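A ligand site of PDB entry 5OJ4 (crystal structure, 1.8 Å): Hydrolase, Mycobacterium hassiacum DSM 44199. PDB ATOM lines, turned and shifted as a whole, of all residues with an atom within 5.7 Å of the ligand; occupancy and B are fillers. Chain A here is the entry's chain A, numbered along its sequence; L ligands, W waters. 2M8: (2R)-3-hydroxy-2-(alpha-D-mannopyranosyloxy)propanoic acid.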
ATOM      1  N   ALA A  33     -11.035  25.330   3.941  1.00  0.00           N
ATOM      2  CA  ALA A  33     -11.648  26.353   4.798  1.00  0.00           C
ATOM      3  C   ALA A  33     -10.756  27.584   4.932  1.00  0.00           C
ATOM      4  O   ALA A  33     -11.269  28.683   5.181  1.00  0.00           O
ATOM      5  CB  ALA A  33     -11.975  25.772   6.187  1.00  0.00           C
ATOM      6  N   TYR A  38      -6.380  25.624   7.810  1.00  0.00           N
ATOM      7  CA  TYR A  38      -7.433  24.632   7.613  1.00  0.00           C
ATOM      8  C   TYR A  38      -7.382  24.160   6.165  1.00  0.00           C
ATOM      9  O   TYR A  38      -8.274  24.472   5.361  1.00  0.00           O
ATOM     10  CB  TYR A  38      -8.811  25.228   7.932  1.00  0.00           C
ATOM     11  CG  TYR A  38      -8.957  25.863   9.311  1.00  0.00           C
ATOM     12  CD1 TYR A  38      -8.715  25.143  10.469  1.00  0.00           C
ATOM     13  CD2 TYR A  38      -9.423  27.187   9.443  1.00  0.00           C
ATOM     14  CE1 TYR A  38      -8.887  25.711  11.744  1.00  0.00           C
ATOM     15  CE2 TYR A  38      -9.608  27.759  10.713  1.00  0.00           C
ATOM     16  CZ  TYR A  38      -9.357  27.035  11.848  1.00  0.00           C
ATOM     17  OH  TYR A  38      -9.530  27.591  13.115  1.00  0.00           O
ATOM     18  N   TRP A  42     -13.962  21.322   5.509  1.00  0.00           N
ATOM     19  CA  TRP A  42     -14.750  21.197   6.741  1.00  0.00           C
ATOM     20  C   TRP A  42     -16.238  21.189   6.399  1.00  0.00           C
ATOM     21  O   TRP A  42     -16.666  21.812   5.425  1.00  0.00           O
ATOM     22  CB  TRP A  42     -14.458  22.369   7.700  1.00  0.00           C
ATOM     23  CG  TRP A  42     -13.440  22.024   8.792  1.00  0.00           C
ATOM     24  CD1 TRP A  42     -13.704  21.773  10.107  1.00  0.00           C
ATOM     25  CD2 TRP A  42     -12.013  21.941   8.633  1.00  0.00           C
ATOM     26  NE1 TRP A  42     -12.528  21.522  10.790  1.00  0.00           N
ATOM     27  CE2 TRP A  42     -11.478  21.607   9.898  1.00  0.00           C
ATOM     28  CE3 TRP A  42     -11.141  22.024   7.531  1.00  0.00           C
ATOM     29  CZ2 TRP A  42     -10.117  21.416  10.104  1.00  0.00           C
ATOM     30  CZ3 TRP A  42      -9.774  21.861   7.744  1.00  0.00           C
ATOM     31  CH2 TRP A  42      -9.284  21.555   9.023  1.00  0.00           C
ATOM     32  N   TRP A  44     -19.385  22.232   8.002  1.00  0.00           N
ATOM     33  CA  TRP A  44     -20.280  23.386   7.888  1.00  0.00           C
ATOM     34  C   TRP A  44     -19.624  24.527   7.097  1.00  0.00           C
ATOM     35  O   TRP A  44     -20.337  25.245   6.382  1.00  0.00           O
ATOM     36  CB  TRP A  44     -20.864  23.866   9.244  1.00  0.00           C
ATOM     37  CG  TRP A  44     -20.034  24.502  10.362  1.00  0.00           C
ATOM     38  CD1 TRP A  44     -18.710  24.337  10.639  1.00  0.00           C
ATOM     39  CD2 TRP A  44     -20.561  25.379  11.381  1.00  0.00           C
ATOM     40  NE1 TRP A  44     -18.375  25.068  11.776  1.00  0.00           N
ATOM     41  CE2 TRP A  44     -19.488  25.727  12.236  1.00  0.00           C
ATOM     42  CE3 TRP A  44     -21.819  25.921  11.638  1.00  0.00           C
ATOM     43  CZ2 TRP A  44     -19.638  26.598  13.320  1.00  0.00           C
ATOM     44  CZ3 TRP A  44     -21.984  26.804  12.732  1.00  0.00           C
ATOM     45  CH2 TRP A  44     -20.892  27.108  13.561  1.00  0.00           C
ATOM     46  N   ASP A  45     -18.280  24.615   7.075  1.00  0.00           N
ATOM     47  CA  ASP A  45     -17.634  25.555   6.153  1.00  0.00           C
ATOM     48  C   ASP A  45     -18.031  25.278   4.705  1.00  0.00           C
ATOM     49  O   ASP A  45     -18.257  26.211   3.921  1.00  0.00           O
ATOM     50  CB  ASP A  45     -16.083  25.517   6.248  1.00  0.00           C
ATOM     51  CG  ASP A  45     -15.565  25.801   7.642  1.00  0.00           C
ATOM     52  OD1 ASP A  45     -15.972  25.056   8.597  1.00  0.00           O
ATOM     53  OD2 ASP A  45     -14.747  26.765   7.789  1.00  0.00           O
ATOM     54  N   HIS A  80     -16.854  15.930  10.076  1.00  0.00           N
ATOM     55  CA  HIS A  80     -16.617  17.365  10.041  1.00  0.00           C
ATOM     56  C   HIS A  80     -15.395  17.754   9.214  1.00  0.00           C
ATOM     57  O   HIS A  80     -15.303  18.929   8.831  1.00  0.00           O
ATOM     58  CB  HIS A  80     -16.562  17.942  11.468  1.00  0.00           C
ATOM     59  CG  HIS A  80     -15.217  17.969  12.110  1.00  0.00           C
ATOM     60  ND1 HIS A  80     -14.455  16.831  12.309  1.00  0.00           N
ATOM     61  CD2 HIS A  80     -14.515  18.995  12.661  1.00  0.00           C
ATOM     62  CE1 HIS A  80     -13.330  17.161  12.926  1.00  0.00           C
ATOM     63  NE2 HIS A  80     -13.338  18.459  13.146  1.00  0.00           N
ATOM     64  N   ILE A  81     -14.471  16.811   8.921  1.00  0.00           N
ATOM     65  CA  ILE A  81     -13.346  17.065   8.013  1.00  0.00           C
ATOM     66  C   ILE A  81     -13.321  16.004   6.929  1.00  0.00           C
ATOM     67  O   ILE A  81     -13.431  14.803   7.222  1.00  0.00           O
ATOM     68  CB  ILE A  81     -11.985  17.108   8.725  1.00  0.00           C
ATOM     69  CG1 ILE A  81     -12.010  18.068   9.906  1.00  0.00           C
ATOM     70  CG2 ILE A  81     -10.854  17.528   7.719  1.00  0.00           C
ATOM     71  CD1 ILE A  81     -10.676  18.038  10.742  1.00  0.00           C
ATOM     72  N   TYR A  90      -2.199  20.088   9.045  1.00  0.00           N
ATOM     73  CA  TYR A  90      -3.291  20.200   9.998  1.00  0.00           C
ATOM     74  C   TYR A  90      -3.228  19.047  10.988  1.00  0.00           C
ATOM     75  O   TYR A  90      -3.050  17.896  10.602  1.00  0.00           O
ATOM     76  CB  TYR A  90      -4.671  20.202   9.326  1.00  0.00           C
ATOM     77  CG  TYR A  90      -5.772  20.308  10.373  1.00  0.00           C
ATOM     78  CD1 TYR A  90      -6.143  21.551  10.890  1.00  0.00           C
ATOM     79  CD2 TYR A  90      -6.374  19.165  10.898  1.00  0.00           C
ATOM     80  CE1 TYR A  90      -7.104  21.641  11.894  1.00  0.00           C
ATOM     81  CE2 TYR A  90      -7.337  19.255  11.888  1.00  0.00           C
ATOM     82  CZ  TYR A  90      -7.713  20.487  12.370  1.00  0.00           C
ATOM     83  OH  TYR A  90      -8.656  20.552  13.372  1.00  0.00           O
ATOM     84  N   PHE A  91      -3.409  19.357  12.280  1.00  0.00           N
ATOM     85  CA  PHE A  91      -3.451  18.320  13.324  1.00  0.00           C
ATOM     86  C   PHE A  91      -4.685  18.579  14.173  1.00  0.00           C
ATOM     87  O   PHE A  91      -4.881  19.721  14.633  1.00  0.00           O
ATOM     88  CB  PHE A  91      -2.207  18.339  14.225  1.00  0.00           C
ATOM     89  CG  PHE A  91      -2.225  17.257  15.271  1.00  0.00           C
ATOM     90  CD1 PHE A  91      -1.745  15.990  14.973  1.00  0.00           C
ATOM     91  CD2 PHE A  91      -2.825  17.466  16.517  1.00  0.00           C
ATOM     92  CE1 PHE A  91      -1.804  14.955  15.905  1.00  0.00           C
ATOM     93  CE2 PHE A  91      -2.889  16.426  17.457  1.00  0.00           C
ATOM     94  CZ  PHE A  91      -2.388  15.177  17.142  1.00  0.00           C
ATOM     95  N   GLN A 117     -20.651  17.890  12.660  1.00  0.00           N
ATOM     96  CA  GLN A 117     -20.694  19.354  12.746  1.00  0.00           C
ATOM     97  C   GLN A 117     -22.110  19.821  12.403  1.00  0.00           C
ATOM     98  O   GLN A 117     -22.920  19.032  11.909  1.00  0.00           O
ATOM     99  CB  GLN A 117     -19.639  20.008  11.814  1.00  0.00           C
ATOM    100  CG  GLN A 117     -18.485  20.649  12.598  1.00  0.00           C
ATOM    101  CD  GLN A 117     -17.546  21.463  11.701  1.00  0.00           C
ATOM    102  OE1 GLN A 117     -17.682  21.448  10.476  1.00  0.00           O
ATOM    103  NE2 GLN A 117     -16.611  22.177  12.318  1.00  0.00           N
ATOM    104  N   TRP A 179     -15.674  20.003  19.378  1.00  0.00           N
ATOM    105  CA  TRP A 179     -15.508  20.382  17.974  1.00  0.00           C
ATOM    106  C   TRP A 179     -16.796  20.216  17.184  1.00  0.00           C
ATOM    107  O   TRP A 179     -16.997  20.909  16.177  1.00  0.00           O
ATOM    108  CB  TRP A 179     -14.398  19.560  17.304  1.00  0.00           C
ATOM    109  CG  TRP A 179     -12.981  20.039  17.558  1.00  0.00           C
ATOM    110  CD1 TRP A 179     -12.557  21.338  17.700  1.00  0.00           C
ATOM    111  CD2 TRP A 179     -11.808  19.225  17.666  1.00  0.00           C
ATOM    112  NE1 TRP A 179     -11.189  21.376  17.910  1.00  0.00           N
ATOM    113  CE2 TRP A 179     -10.708  20.099  17.890  1.00  0.00           C
ATOM    114  CE3 TRP A 179     -11.567  17.843  17.588  1.00  0.00           C
ATOM    115  CZ2 TRP A 179      -9.395  19.618  18.048  1.00  0.00           C
ATOM    116  CZ3 TRP A 179     -10.263  17.378  17.762  1.00  0.00           C
ATOM    117  CH2 TRP A 179      -9.188  18.259  17.975  1.00  0.00           C
ATOM    118  N   GLY A 182     -18.898  23.241  16.581  1.00  0.00           N
ATOM    119  CA  GLY A 182     -18.217  24.316  15.871  1.00  0.00           C
ATOM    120  C   GLY A 182     -17.398  25.222  16.760  1.00  0.00           C
ATOM    121  O   GLY A 182     -16.593  25.988  16.247  1.00  0.00           O
ATOM    122  N   MET A 183     -17.575  25.155  18.101  1.00  0.00           N
ATOM    123  CA  MET A 183     -17.014  26.153  19.031  1.00  0.00           C
ATOM    124  C   MET A 183     -16.311  25.421  20.184  1.00  0.00           C
ATOM    125  O   MET A 183     -16.789  25.398  21.321  1.00  0.00           O
ATOM    126  CB  MET A 183     -18.115  27.071  19.580  1.00  0.00           C
ATOM    127  CG  MET A 183     -19.161  27.500  18.544  1.00  0.00           C
ATOM    128  SD  MET A 183     -20.410  28.535  19.368  1.00  0.00           S
ATOM    129  CE  MET A 183     -21.526  28.819  18.003  1.00  0.00           C
ATOM    130  N   ASP A 208      -1.791  23.936  14.682  1.00  0.00           N
ATOM    131  CA  ASP A 208      -2.597  25.157  14.556  1.00  0.00           C
ATOM    132  C   ASP A 208      -1.847  26.385  15.069  1.00  0.00           C
ATOM    133  O   ASP A 208      -1.954  27.466  14.477  1.00  0.00           O
ATOM    134  CB  ASP A 208      -3.930  24.984  15.297  1.00  0.00           C
ATOM    135  CG  ASP A 208      -3.740  24.790  16.809  1.00  0.00           C
ATOM    136  OD1 ASP A 208      -3.067  23.796  17.217  1.00  0.00           O
ATOM    137  OD2 ASP A 208      -4.252  25.636  17.575  1.00  0.00           O
ATOM    138  N   ARG A 218      -5.623  31.220  20.168  1.00  0.00           N
ATOM    139  CA  ARG A 218      -5.986  29.815  20.030  1.00  0.00           C
ATOM    140  C   ARG A 218      -6.121  29.176  21.410  1.00  0.00           C
ATOM    141  O   ARG A 218      -5.690  29.745  22.422  1.00  0.00           O
ATOM    142  CB  ARG A 218      -4.935  29.045  19.212  1.00  0.00           C
ATOM    143  CG  ARG A 218      -4.701  29.577  17.779  1.00  0.00           C
ATOM    144  CD  ARG A 218      -5.784  29.150  16.796  1.00  0.00           C
ATOM    145  NE  ARG A 218      -6.073  27.702  16.832  1.00  0.00           N
ATOM    146  CZ  ARG A 218      -7.080  27.155  16.150  1.00  0.00           C
ATOM    147  NH1 ARG A 218      -7.858  27.929  15.402  1.00  0.00           N
ATOM    148  NH2 ARG A 218      -7.315  25.842  16.216  1.00  0.00           N
ATOM    149  N   TYR A 224      -6.205  21.314  24.354  1.00  0.00           N
ATOM    150  CA  TYR A 224      -5.945  20.347  23.294  1.00  0.00           C
ATOM    151  C   TYR A 224      -5.774  18.940  23.870  1.00  0.00           C
ATOM    152  O   TYR A 224      -6.196  17.954  23.248  1.00  0.00           O
ATOM    153  CB  TYR A 224      -4.723  20.761  22.468  1.00  0.00           C
ATOM    154  CG  TYR A 224      -5.164  21.415  21.182  1.00  0.00           C
ATOM    155  CD1 TYR A 224      -5.639  22.726  21.172  1.00  0.00           C
ATOM    156  CD2 TYR A 224      -5.182  20.699  19.983  1.00  0.00           C
ATOM    157  CE1 TYR A 224      -6.091  23.344  20.001  1.00  0.00           C
ATOM    158  CE2 TYR A 224      -5.638  21.318  18.784  1.00  0.00           C
ATOM    159  CZ  TYR A 224      -6.089  22.628  18.813  1.00  0.00           C
ATOM    160  OH  TYR A 224      -6.551  23.226  17.650  1.00  0.00           O
ATOM    161  N   TYR A 377     -10.482  33.015  19.968  1.00  0.00           N
ATOM    162  CA  TYR A 377     -11.217  32.006  19.200  1.00  0.00           C
ATOM    163  C   TYR A 377     -12.713  32.122  19.478  1.00  0.00           C
ATOM    164  O   TYR A 377     -13.311  33.133  19.073  1.00  0.00           O
ATOM    165  CB  TYR A 377     -10.600  30.621  19.523  1.00  0.00           C
ATOM    166  CG  TYR A 377     -10.950  29.363  18.714  1.00  0.00           C
ATOM    167  CD1 TYR A 377     -11.105  29.355  17.328  1.00  0.00           C
ATOM    168  CD2 TYR A 377     -11.026  28.137  19.387  1.00  0.00           C
ATOM    169  CE1 TYR A 377     -11.391  28.128  16.638  1.00  0.00           C
ATOM    170  CE2 TYR A 377     -11.300  26.962  18.747  1.00  0.00           C
ATOM    171  CZ  TYR A 377     -11.473  26.937  17.392  1.00  0.00           C
ATOM    172  OH  TYR A 377     -11.771  25.694  16.854  1.00  0.00           O
ATOM    173  N   TRP A 378     -13.361  31.163  20.156  1.00  0.00           N
ATOM    174  CA  TRP A 378     -14.798  31.302  20.404  1.00  0.00           C
ATOM    175  C   TRP A 378     -15.131  31.876  21.781  1.00  0.00           C
ATOM    176  O   TRP A 378     -16.302  31.853  22.186  1.00  0.00           O
ATOM    177  CB  TRP A 378     -15.514  29.957  20.220  1.00  0.00           C
ATOM    178  CG  TRP A 378     -15.522  29.467  18.766  1.00  0.00           C
ATOM    179  CD1 TRP A 378     -14.594  28.653  18.174  1.00  0.00           C
ATOM    180  CD2 TRP A 378     -16.476  29.811  17.751  1.00  0.00           C
ATOM    181  NE1 TRP A 378     -14.921  28.448  16.860  1.00  0.00           N
ATOM    182  CE2 TRP A 378     -16.083  29.143  16.577  1.00  0.00           C
ATOM    183  CE3 TRP A 378     -17.638  30.611  17.720  1.00  0.00           C
ATOM    184  CZ2 TRP A 378     -16.796  29.227  15.377  1.00  0.00           C
ATOM    185  CZ3 TRP A 378     -18.351  30.719  16.520  1.00  0.00           C
ATOM    186  CH2 TRP A 378     -17.937  30.038  15.365  1.00  0.00           C
ATOM    187  N   TRP A 383     -17.465  36.691  14.912  1.00  0.00           N
ATOM    188  CA  TRP A 383     -17.254  35.756  13.803  1.00  0.00           C
ATOM    189  C   TRP A 383     -18.156  36.109  12.630  1.00  0.00           C
ATOM    190  O   TRP A 383     -19.392  36.058  12.786  1.00  0.00           O
ATOM    191  CB  TRP A 383     -17.546  34.327  14.248  1.00  0.00           C
ATOM    192  CG  TRP A 383     -16.531  33.759  15.135  1.00  0.00           C
ATOM    193  CD1 TRP A 383     -16.296  34.084  16.437  1.00  0.00           C
ATOM    194  CD2 TRP A 383     -15.619  32.714  14.791  1.00  0.00           C
ATOM    195  NE1 TRP A 383     -15.264  33.304  16.931  1.00  0.00           N
ATOM    196  CE2 TRP A 383     -14.838  32.461  15.949  1.00  0.00           C
ATOM    197  CE3 TRP A 383     -15.358  31.998  13.615  1.00  0.00           C
ATOM    198  CZ2 TRP A 383     -13.826  31.479  15.970  1.00  0.00           C
ATOM    199  CZ3 TRP A 383     -14.369  31.024  13.640  1.00  0.00           C
ATOM    200  CH2 TRP A 383     -13.604  30.770  14.814  1.00  0.00           C
ATOM    201  N   GLU A 421     -10.930  35.134   9.851  1.00  0.00           N
ATOM    202  CA  GLU A 421     -11.725  34.107  10.508  1.00  0.00           C
ATOM    203  C   GLU A 421     -12.611  34.698  11.618  1.00  0.00           C
ATOM    204  O   GLU A 421     -13.782  34.338  11.744  1.00  0.00           O
ATOM    205  CB  GLU A 421     -10.742  33.059  11.069  1.00  0.00           C
ATOM    206  CG  GLU A 421     -11.399  31.764  11.592  1.00  0.00           C
ATOM    207  CD  GLU A 421     -10.397  30.873  12.303  1.00  0.00           C
ATOM    208  OE1 GLU A 421      -9.179  31.185  12.334  1.00  0.00           O
ATOM    209  OE2 GLU A 421     -10.841  29.819  12.842  1.00  0.00           O
ATOM    210  N   GLN A 436     -10.160  33.431   5.146  1.00  0.00           N
ATOM    211  CA  GLN A 436     -11.050  32.362   5.594  1.00  0.00           C
ATOM    212  C   GLN A 436     -12.220  32.232   4.623  1.00  0.00           C
ATOM    213  O   GLN A 436     -12.925  33.209   4.355  1.00  0.00           O
ATOM    214  CB  GLN A 436     -11.539  32.680   7.018  1.00  0.00           C
ATOM    215  CG  GLN A 436     -12.415  31.594   7.672  1.00  0.00           C
ATOM    216  CD  GLN A 436     -11.626  30.389   8.158  1.00  0.00           C
ATOM    217  OE1 GLN A 436     -10.407  30.467   8.277  1.00  0.00           O
ATOM    218  NE2 GLN A 436     -12.319  29.282   8.469  1.00  0.00           N
ATOM    219  N   TRP A 438     -15.282  30.932   4.613  1.00  0.00           N
ATOM    220  CA  TRP A 438     -16.668  31.255   4.878  1.00  0.00           C
ATOM    221  C   TRP A 438     -16.873  32.735   5.175  1.00  0.00           C
ATOM    222  O   TRP A 438     -17.993  33.227   5.060  1.00  0.00           O
ATOM    223  CB  TRP A 438     -17.255  30.380   6.014  1.00  0.00           C
ATOM    224  CG  TRP A 438     -16.647  30.446   7.391  1.00  0.00           C
ATOM    225  CD1 TRP A 438     -15.773  31.366   7.907  1.00  0.00           C
ATOM    226  CD2 TRP A 438     -16.912  29.494   8.441  1.00  0.00           C
ATOM    227  NE1 TRP A 438     -15.489  31.038   9.245  1.00  0.00           N
ATOM    228  CE2 TRP A 438     -16.162  29.895   9.574  1.00  0.00           C
ATOM    229  CE3 TRP A 438     -17.754  28.369   8.538  1.00  0.00           C
ATOM    230  CZ2 TRP A 438     -16.195  29.176  10.802  1.00  0.00           C
ATOM    231  CZ3 TRP A 438     -17.789  27.662   9.759  1.00  0.00           C
ATOM    232  CH2 TRP A 438     -17.003  28.056  10.857  1.00  0.00           C
HETATM  233  C1  2M8 L   1     -12.412  25.516  13.757  1.00  0.00           C
HETATM  234  O1  2M8 L   1     -12.296  24.196  14.221  1.00  0.00           O
HETATM  235  C22 2M8 L   1     -11.237  23.351  13.830  1.00  0.00           C
HETATM  236  C23 2M8 L   1     -11.601  21.882  14.184  1.00  0.00           C
HETATM  237  O13 2M8 L   1     -12.849  21.528  13.635  1.00  0.00           O
HETATM  238  C21 2M8 L   1      -9.926  23.720  14.527  1.00  0.00           C
HETATM  239  O1A 2M8 L   1      -8.938  22.976  14.307  1.00  0.00           O
HETATM  240  O1B 2M8 L   1      -9.818  24.692  15.317  1.00  0.00           O
HETATM  241  C2  2M8 L   1     -13.833  25.987  14.123  1.00  0.00           C
HETATM  242  O2  2M8 L   1     -13.869  27.401  14.057  1.00  0.00           O
HETATM  243  C3  2M8 L   1     -14.861  25.387  13.257  1.00  0.00           C
HETATM  244  O3  2M8 L   1     -16.142  25.932  13.553  1.00  0.00           O
HETATM  245  C4  2M8 L   1     -14.551  25.492  11.796  1.00  0.00           C
HETATM  246  O4  2M8 L   1     -15.455  24.662  11.093  1.00  0.00           O
HETATM  247  C5  2M8 L   1     -13.120  25.000  11.450  1.00  0.00           C
HETATM  248  C6  2M8 L   1     -12.691  25.303   9.990  1.00  0.00           C
HETATM  249  O6  2M8 L   1     -12.951  26.657   9.706  1.00  0.00           O
HETATM  250  O5  2M8 L   1     -12.121  25.616  12.321  1.00  0.00           O
HETATM  251  O   HOH W   1      -6.411  22.168  15.269  1.00  0.00           O
HETATM  252  O   HOH W   2     -13.017  28.637  11.822  1.00  0.00           O
HETATM  253  O   HOH W   3     -15.068  22.477  15.139  1.00  0.00           O
HETATM  254  O   HOH W   4      -9.549  23.713  18.139  1.00  0.00           O
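Residues that only touch the ligand: Trp 383, Trp 438, Trp 179 and Ala 33.
Hydrophobic or aromatic side chains that line the ligand: Ala 33, Tyr 38, Trp 42, Trp 44, His 80, Tyr 90, Trp 179, Tyr 377, Trp 378, Trp 383 and Trp 438.
Of the 22 residues printed, 16 come within 4 Å of the ligand.
The nearest printed residue that does not touch the ligand is Glu 421 (4.1 Å).
The backbone carbonyl oxygen of Tyr 377 sits at hydrogen-bond distance from the indole nitrogen of Trp 383 (2.9 Å).
O of Gly 182 lies within hydrogen-bond range of NE1 of Trp 378.
NH1 of Arg 218 sits at hydrogen-bond distance from OH of Tyr 38 (2.9 Å).
The side-chain hydroxyl (OH) of Tyr 224 lies within hydrogen-bond range of the guanidinium group (NH2) of Arg 218 (3.1 Å).
NE of Arg 218 lies within salt-bridge range of OD2 of Asp 208, at 2.9 Å.
The side-chain amide oxygen (OE1) of Gln 117 sits close to the backbone NH (N) of Trp 44 (3.1 Å).
The backbone NH of Ala 33 is in hydrogen-bond range of the backbone carbonyl oxygen of Tyr 38, 3.2 Å away.
The side-chain hydroxyl (OH) of Tyr 38 is in hydrogen-bond range of the side-chain carboxylate (OE2) of Glu 421 (2.6 Å).
An oxygen (O4) of the ligand sits at hydrogen-bond distance from the side-chain carboxylate of Asp 45, 2.6 Å away.
An oxygen (O1A) of the ligand is in hydrogen-bond range of the side-chain hydroxyl (OH) of Tyr 90.
An oxygen (O1B) of the ligand is in hydrogen-bond range of the side-chain hydroxyl (OH) of Tyr 377, at 2.7 Å.
The backbone carbonyl oxygen (O) of Gly 182 is in hydrogen-bond range of an oxygen (O3) of the ligand, 2.7 Å away.
The indole nitrogen (NE1) of Trp 42 is in hydrogen-bond range of an oxygen (O13) of the ligand (2.9 Å).
The guanidinium group (NH2) of Arg 218 is in salt-bridge range of an oxygen (O1B) of the ligand (2.9 Å).
An oxygen (O6) of the ligand sits at hydrogen-bond distance from the side-chain amide nitrogen (NE2) of Gln 436 (3.0 Å).
An oxygen (O3) of the ligand lies within hydrogen-bond range of the indole nitrogen (NE1) of Trp 44.
The side-chain amide nitrogen (NE2) of Gln 117 sits at hydrogen-bond distance from an oxygen (O4) of the ligand, 3.0 Å away.
O5 of the ligand sits close to OH of Tyr 38 (3.4 Å).
A ring nitrogen (NE2) of His 80 is in hydrogen-bond range of an oxygen (O13) of the ligand (3.1 Å).
O2 of the ligand lies within hydrogen-bond range of NE1 of Trp 378 (3.2 Å).
Water W2 lies within hydrogen-bond range of the side-chain carboxylate (OE2) of Glu 421, an oxygen (O2) of the ligand and the side-chain amide nitrogen (NE2) of Gln 436.
Water W1 lies within hydrogen-bond range of the side-chain hydroxyl (OH) of Tyr 224, an oxygen (O1A) of the ligand, the backbone carbonyl oxygen (O) of Phe 91 and the side-chain hydroxyl (OH) of Tyr 90.
Water W3 lies within hydrogen-bond range of O of Trp 179 (2.7 Å), O13 of the ligand (2.8 Å) and NE2 of Gln 117 (3.2 Å).
Water W4 lies within hydrogen-bond range of NE1 of Trp 179 (2.9 Å), O1B of the ligand (3.0 Å), OH of Tyr 224 (3.1 Å) and OH of Tyr 377 (3.2 Å).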
